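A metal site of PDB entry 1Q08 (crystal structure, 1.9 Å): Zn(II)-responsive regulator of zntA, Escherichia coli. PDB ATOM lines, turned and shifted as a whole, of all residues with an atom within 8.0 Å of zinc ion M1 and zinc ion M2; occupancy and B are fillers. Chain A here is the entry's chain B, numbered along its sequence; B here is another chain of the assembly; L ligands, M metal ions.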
ATOM      1  N   LEU A  68      36.702  -6.749   4.574  1.00  0.00           N
ATOM      2  CA  LEU A  68      35.432  -6.320   3.979  1.00  0.00           C
ATOM      3  C   LEU A  68      35.681  -5.102   3.097  1.00  0.00           C
ATOM      4  O   LEU A  68      35.176  -5.007   1.978  1.00  0.00           O
ATOM      5  CB  LEU A  68      34.423  -5.960   5.070  1.00  0.00           C
ATOM      6  CG  LEU A  68      33.845  -7.095   5.920  1.00  0.00           C
ATOM      7  CD1 LEU A  68      32.994  -6.517   7.030  1.00  0.00           C
ATOM      8  CD2 LEU A  68      33.008  -8.023   5.047  1.00  0.00           C
ATOM      9  N   ASN A  69      36.464  -4.172   3.633  1.00  0.00           N
ATOM     10  CA  ASN A  69      36.805  -2.955   2.932  1.00  0.00           C
ATOM     11  C   ASN A  69      37.520  -3.203   1.603  1.00  0.00           C
ATOM     12  O   ASN A  69      37.100  -2.704   0.547  1.00  0.00           O
ATOM     13  CB  ASN A  69      37.712  -2.092   3.802  1.00  0.00           C
ATOM     14  CG  ASN A  69      38.121  -0.809   3.108  1.00  0.00           C
ATOM     15  OD1 ASN A  69      37.395   0.184   3.134  1.00  0.00           O
ATOM     16  ND2 ASN A  69      39.290  -0.833   2.469  1.00  0.00           N
ATOM     17  N   ALA A  71      37.720  -5.789  -0.413  1.00  0.00           N
ATOM     18  CA  ALA A  71      37.069  -6.543  -1.487  1.00  0.00           C
ATOM     19  C   ALA A  71      36.000  -5.757  -2.249  1.00  0.00           C
ATOM     20  O   ALA A  71      35.633  -6.142  -3.365  1.00  0.00           O
ATOM     21  CB  ALA A  71      36.457  -7.827  -0.923  1.00  0.00           C
ATOM     22  N   CYS A  72      35.518  -4.670  -1.660  1.00  0.00           N
ATOM     23  CA  CYS A  72      34.466  -3.870  -2.279  1.00  0.00           C
ATOM     24  C   CYS A  72      35.004  -2.742  -3.150  1.00  0.00           C
ATOM     25  O   CYS A  72      35.948  -2.038  -2.771  1.00  0.00           O
ATOM     26  CB  CYS A  72      33.557  -3.302  -1.177  1.00  0.00           C
ATOM     27  SG  CYS A  72      32.199  -2.275  -1.771  1.00  0.00           S
ATOM     28  N   CYS A  73      34.405  -2.562  -4.334  1.00  0.00           N
ATOM     29  CA  CYS A  73      34.839  -1.511  -5.251  1.00  0.00           C
ATOM     30  C   CYS A  73      34.519  -0.117  -4.714  1.00  0.00           C
ATOM     31  O   CYS A  73      35.184   0.863  -5.078  1.00  0.00           O
ATOM     32  CB  CYS A  73      34.166  -1.676  -6.618  1.00  0.00           C
ATOM     33  SG  CYS A  73      32.429  -1.142  -6.685  1.00  0.00           S
ATOM     34  N   GLY A  74      33.508  -0.038  -3.860  1.00  0.00           N
ATOM     35  CA  GLY A  74      33.123   1.234  -3.268  1.00  0.00           C
ATOM     36  C   GLY A  74      32.592   2.298  -4.232  1.00  0.00           C
ATOM     37  O   GLY A  74      32.695   3.491  -3.944  1.00  0.00           O
ATOM     38  N   THR A  75      32.024   1.873  -5.356  1.00  0.00           N
ATOM     39  CA  THR A  75      31.501   2.824  -6.339  1.00  0.00           C
ATOM     40  C   THR A  75      29.991   2.706  -6.531  1.00  0.00           C
ATOM     41  O   THR A  75      29.307   2.054  -5.740  1.00  0.00           O
ATOM     42  CB  THR A  75      32.195   2.637  -7.707  1.00  0.00           C
ATOM     43  OG1 THR A  75      31.808   1.378  -8.270  1.00  0.00           O
ATOM     44  CG2 THR A  75      33.713   2.643  -7.534  1.00  0.00           C
ATOM     45  N   ALA A  76      29.472   3.347  -7.572  1.00  0.00           N
ATOM     46  CA  ALA A  76      28.038   3.313  -7.870  1.00  0.00           C
ATOM     47  C   ALA A  76      27.526   1.902  -8.144  1.00  0.00           C
ATOM     48  O   ALA A  76      26.315   1.671  -8.235  1.00  0.00           O
ATOM     49  CB  ALA A  76      27.735   4.226  -9.056  1.00  0.00           C
ATOM     50  N   HIS A  77      28.454   0.957  -8.296  1.00  0.00           N
ATOM     51  CA  HIS A  77      28.144  -0.460  -8.533  1.00  0.00           C
ATOM     52  C   HIS A  77      26.946  -0.842  -7.656  1.00  0.00           C
ATOM     53  O   HIS A  77      26.965  -0.612  -6.452  1.00  0.00           O
ATOM     54  CB  HIS A  77      29.369  -1.306  -8.146  1.00  0.00           C
ATOM     55  CG  HIS A  77      29.351  -2.710  -8.674  1.00  0.00           C
ATOM     56  ND1 HIS A  77      30.042  -3.728  -8.060  1.00  0.00           N
ATOM     57  CD2 HIS A  77      28.779  -3.246  -9.773  1.00  0.00           C
ATOM     58  CE1 HIS A  77      29.888  -4.844  -8.755  1.00  0.00           C
ATOM     59  NE2 HIS A  77      29.123  -4.570  -9.803  1.00  0.00           N
ATOM     60  N   SER A  78      25.923  -1.437  -8.258  1.00  0.00           N
ATOM     61  CA  SER A  78      24.718  -1.831  -7.508  1.00  0.00           C
ATOM     62  C   SER A  78      25.042  -2.789  -6.368  1.00  0.00           C
ATOM     63  O   SER A  78      25.759  -3.776  -6.544  1.00  0.00           O
ATOM     64  CB  SER A  78      23.699  -2.485  -8.443  1.00  0.00           C
ATOM     65  OG  SER A  78      22.582  -2.949  -7.720  1.00  0.00           O
ATOM     66  N   SER A  79      24.487  -2.501  -5.186  1.00  0.00           N
ATOM     67  CA  SER A  79      24.745  -3.340  -4.014  1.00  0.00           C
ATOM     68  C   SER A  79      24.217  -4.756  -4.192  1.00  0.00           C
ATOM     69  O   SER A  79      24.417  -5.617  -3.329  1.00  0.00           O
ATOM     70  CB  SER A  79      24.159  -2.705  -2.748  1.00  0.00           C
ATOM     71  OG  SER A  79      22.753  -2.672  -2.783  1.00  0.00           O
ATOM     72  N   VAL A  80      23.530  -5.017  -5.301  1.00  0.00           N
ATOM     73  CA  VAL A  80      23.030  -6.362  -5.564  1.00  0.00           C
ATOM     74  C   VAL A  80      24.234  -7.296  -5.659  1.00  0.00           C
ATOM     75  O   VAL A  80      24.146  -8.482  -5.344  1.00  0.00           O
ATOM     76  CB  VAL A  80      22.255  -6.415  -6.911  1.00  0.00           C
ATOM     77  CG1 VAL A  80      22.085  -7.865  -7.370  1.00  0.00           C
ATOM     78  CG2 VAL A  80      20.897  -5.745  -6.761  1.00  0.00           C
ATOM     79  N   TYR A  81      25.368  -6.732  -6.054  1.00  0.00           N
ATOM     80  CA  TYR A  81      26.602  -7.500  -6.221  1.00  0.00           C
ATOM     81  C   TYR A  81      27.635  -7.274  -5.122  1.00  0.00           C
ATOM     82  O   TYR A  81      28.741  -7.807  -5.201  1.00  0.00           O
ATOM     83  CB  TYR A  81      27.260  -7.153  -7.555  1.00  0.00           C
ATOM     84  CG  TYR A  81      26.320  -7.157  -8.737  1.00  0.00           C
ATOM     85  CD1 TYR A  81      25.802  -5.974  -9.252  1.00  0.00           C
ATOM     86  CD2 TYR A  81      25.947  -8.354  -9.351  1.00  0.00           C
ATOM     87  CE1 TYR A  81      24.928  -5.977 -10.345  1.00  0.00           C
ATOM     88  CE2 TYR A  81      25.082  -8.378 -10.436  1.00  0.00           C
ATOM     89  CZ  TYR A  81      24.582  -7.179 -10.929  1.00  0.00           C
ATOM     90  OH  TYR A  81      23.734  -7.205 -12.013  1.00  0.00           O
ATOM     91  N   CYS A  82      27.286  -6.505  -4.097  1.00  0.00           N
ATOM     92  CA  CYS A  82      28.251  -6.207  -3.044  1.00  0.00           C
ATOM     93  C   CYS A  82      28.757  -7.368  -2.210  1.00  0.00           C
ATOM     94  O   CYS A  82      27.986  -8.122  -1.617  1.00  0.00           O
ATOM     95  CB  CYS A  82      27.707  -5.125  -2.113  1.00  0.00           C
ATOM     96  SG  CYS A  82      28.990  -4.500  -1.024  1.00  0.00           S
ATOM     97  N   SER A  83      30.085  -7.475  -2.141  1.00  0.00           N
ATOM     98  CA  SER A  83      30.766  -8.529  -1.397  1.00  0.00           C
ATOM     99  C   SER A  83      30.616  -8.349   0.117  1.00  0.00           C
ATOM    100  O   SER A  83      30.736  -9.313   0.874  1.00  0.00           O
ATOM    101  CB  SER A  83      32.249  -8.531  -1.753  1.00  0.00           C
ATOM    102  OG  SER A  83      32.818  -7.264  -1.492  1.00  0.00           O
ATOM    103  N   ILE A  84      30.386  -7.109   0.548  1.00  0.00           N
ATOM    104  CA  ILE A  84      30.215  -6.827   1.970  1.00  0.00           C
ATOM    105  C   ILE A  84      28.948  -7.526   2.478  1.00  0.00           C
ATOM    106  O   ILE A  84      28.971  -8.199   3.513  1.00  0.00           O
ATOM    107  CB  ILE A  84      30.098  -5.309   2.229  1.00  0.00           C
ATOM    108  CG1 ILE A  84      31.422  -4.612   1.876  1.00  0.00           C
ATOM    109  CG2 ILE A  84      29.731  -5.043   3.697  1.00  0.00           C
ATOM    110  CD1 ILE A  84      31.377  -3.091   1.966  1.00  0.00           C
ATOM    111  N   LEU A  85      27.852  -7.358   1.744  1.00  0.00           N
ATOM    112  CA  LEU A  85      26.591  -7.985   2.121  1.00  0.00           C
ATOM    113  C   LEU A  85      26.709  -9.504   2.090  1.00  0.00           C
ATOM    114  O   LEU A  85      26.181 -10.203   2.951  1.00  0.00           O
ATOM    115  CB  LEU A  85      25.473  -7.526   1.169  1.00  0.00           C
ATOM    116  CG  LEU A  85      25.038  -6.062   1.307  1.00  0.00           C
ATOM    117  CD1 LEU A  85      24.123  -5.698   0.145  1.00  0.00           C
ATOM    118  CD2 LEU A  85      24.300  -5.863   2.630  1.00  0.00           C
ATOM    119  N   GLU A  86      27.416 -10.024   1.082  1.00  0.00           N
ATOM    120  CA  GLU A  86      27.609 -11.463   0.958  1.00  0.00           C
ATOM    121  C   GLU A  86      28.374 -11.991   2.174  1.00  0.00           C
ATOM    122  O   GLU A  86      27.998 -13.007   2.760  1.00  0.00           O
ATOM    123  CB  GLU A  86      28.407 -11.802  -0.308  1.00  0.00           C
ATOM    124  CG  GLU A  86      27.745 -11.331  -1.598  1.00  0.00           C
ATOM    125  CD  GLU A  86      28.536 -11.736  -2.829  1.00  0.00           C
ATOM    126  OE1 GLU A  86      29.763 -11.518  -2.856  1.00  0.00           O
ATOM    127  OE2 GLU A  86      27.923 -12.259  -3.782  1.00  0.00           O
ATOM    128  N   THR B  36      24.174   1.145  -3.351  1.00  0.00           N
ATOM    129  CA  THR B  36      25.433   0.879  -4.015  1.00  0.00           C
ATOM    130  C   THR B  36      26.578   0.439  -3.108  1.00  0.00           C
ATOM    131  O   THR B  36      26.477   0.498  -1.879  1.00  0.00           O
ATOM    132  CB  THR B  36      25.918   2.140  -4.756  1.00  0.00           C
ATOM    133  OG1 THR B  36      26.314   3.111  -3.787  1.00  0.00           O
ATOM    134  CG2 THR B  36      24.805   2.707  -5.613  1.00  0.00           C
ATOM    135  N   CYS B  37      27.670   0.002  -3.728  1.00  0.00           N
ATOM    136  CA  CYS B  37      28.847  -0.433  -2.999  1.00  0.00           C
ATOM    137  C   CYS B  37      29.452   0.752  -2.272  1.00  0.00           C
ATOM    138  O   CYS B  37      30.117   0.593  -1.242  1.00  0.00           O
ATOM    139  CB  CYS B  37      29.875  -1.034  -3.959  1.00  0.00           C
ATOM    140  SG  CYS B  37      29.457  -2.695  -4.488  1.00  0.00           S
ATOM    141  N   GLN B  38      29.249   1.946  -2.804  1.00  0.00           N
ATOM    142  CA  GLN B  38      29.788   3.131  -2.167  1.00  0.00           C
ATOM    143  C   GLN B  38      29.152   3.314  -0.789  1.00  0.00           C
ATOM    144  O   GLN B  38      29.833   3.695   0.168  1.00  0.00           O
ATOM    145  CB  GLN B  38      29.535   4.378  -3.032  1.00  0.00           C
ATOM    146  CG  GLN B  38      30.127   5.655  -2.461  1.00  0.00           C
ATOM    147  CD  GLN B  38      30.114   6.811  -3.441  1.00  0.00           C
ATOM    148  OE1 GLN B  38      30.568   7.911  -3.123  1.00  0.00           O
ATOM    149  NE2 GLN B  38      29.601   6.570  -4.642  1.00  0.00           N
ATOM    150  N   GLU B  39      27.858   3.028  -0.687  1.00  0.00           N
ATOM    151  CA  GLU B  39      27.141   3.164   0.569  1.00  0.00           C
ATOM    152  C   GLU B  39      27.566   2.103   1.578  1.00  0.00           C
ATOM    153  O   GLU B  39      27.844   2.417   2.736  1.00  0.00           O
ATOM    154  CB  GLU B  39      25.629   3.069   0.339  1.00  0.00           C
ATOM    155  CG  GLU B  39      25.083   4.098  -0.624  1.00  0.00           C
ATOM    156  CD  GLU B  39      23.603   3.883  -0.911  1.00  0.00           C
ATOM    157  OE1 GLU B  39      22.763   4.260  -0.066  1.00  0.00           O
ATOM    158  OE2 GLU B  39      23.287   3.315  -1.971  1.00  0.00           O
ATOM    159  N   SER B  40      27.616   0.850   1.135  1.00  0.00           N
ATOM    160  CA  SER B  40      28.009  -0.232   2.036  1.00  0.00           C
ATOM    161  C   SER B  40      29.470  -0.096   2.451  1.00  0.00           C
ATOM    162  O   SER B  40      29.808  -0.281   3.628  1.00  0.00           O
ATOM    163  CB  SER B  40      27.787  -1.591   1.349  1.00  0.00           C
ATOM    164  OG  SER B  40      28.473  -1.669   0.121  1.00  0.00           O
ATOM    165  N   LYS B  41      30.343   0.257   1.515  1.00  0.00           N
ATOM    166  CA  LYS B  41      31.751   0.408   1.856  1.00  0.00           C
ATOM    167  C   LYS B  41      31.955   1.576   2.825  1.00  0.00           C
ATOM    168  O   LYS B  41      32.798   1.514   3.717  1.00  0.00           O
ATOM    169  CB  LYS B  41      32.596   0.613   0.604  1.00  0.00           C
ATOM    170  CG  LYS B  41      34.094   0.640   0.897  1.00  0.00           C
ATOM    171  CD  LYS B  41      34.939   0.450  -0.354  1.00  0.00           C
ATOM    172  CE  LYS B  41      36.415   0.404   0.009  1.00  0.00           C
ATOM    173  NZ  LYS B  41      37.290  -0.043  -1.118  1.00  0.00           N
HETATM  174  P1  LIG L   1      31.856  -5.689  -4.949  1.00  0.00           P
HETATM  175  O1  LIG L   1      30.551  -5.841  -5.647  1.00  0.00           O
HETATM  176  O2  LIG L   1      32.569  -4.502  -5.474  1.00  0.00           O
HETATM  177  O3  LIG L   1      31.620  -5.532  -3.497  1.00  0.00           O
HETATM  178  O4  LIG L   1      32.683  -6.896  -5.178  1.00  0.00           O
HETATM  179 ZN    ZN M   1      31.150  -3.043  -6.188  1.00  0.00          ZN
HETATM  180 ZN    ZN M   2      30.670  -3.779  -2.698  1.00  0.00          ZN
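OG1 of Thr 75 sits close to N of His 77 (3.4 Å). SG of Cys 72 lies close to N of Gly 74. NZ of Lys 41 of chain B sits at hydrogen-bond distance from O of Cys 72 (2.9 Å). OG1 of Thr 75 lies close to SG of Cys 73 (3.0 Å). O of Cys 37 of chain B is in hydrogen-bond range of OG of Ser 40 of chain B (3.1 Å). The backbone NH of Cys 37 of chain B sits at hydrogen-bond distance from the backbone carbonyl oxygen of Thr 75. SG of Cys 82 sits close to OG of Ser 40 of chain B (3.1 Å). N of Ile 84 sits close to SG of Cys 82.
The nearest printed residue that does not touch zinc ion M1 is Gly 74 (4.5 Å).
Ser 83 touches zinc ion M2. Within 4 Å of zinc ion M2: Cys 72, Cys 82, Ser 83 and Cys 37 of chain B. The nearest printed residue that does not touch zinc ion M2 is Ser 40 of chain B (4.2 Å).
Zinc ion M1 is bound by an oxygen (O2) of the ligand (2.2 Å), a ring nitrogen (ND1) of His 77 (2.3 Å), the side-chain sulfur (SG) of Cys 73 (2.3 Å) and the side-chain sulfur (SG) of Cys 37 of chain B (2.4 Å).
Zinc ion M2 is bound by O3 of the ligand (2.1 Å). Zinc ion M2 is bound by SG of Cys 72, 2.3 Å away. SG of Cys 37 of chain B binds zinc ion M2, at 2.4 Å. Zinc ion M2 is bound by the side-chain sulfur (SG) of Cys 82, 2.5 Å away. Zinc ion M2 has four donor atoms within binding distance.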
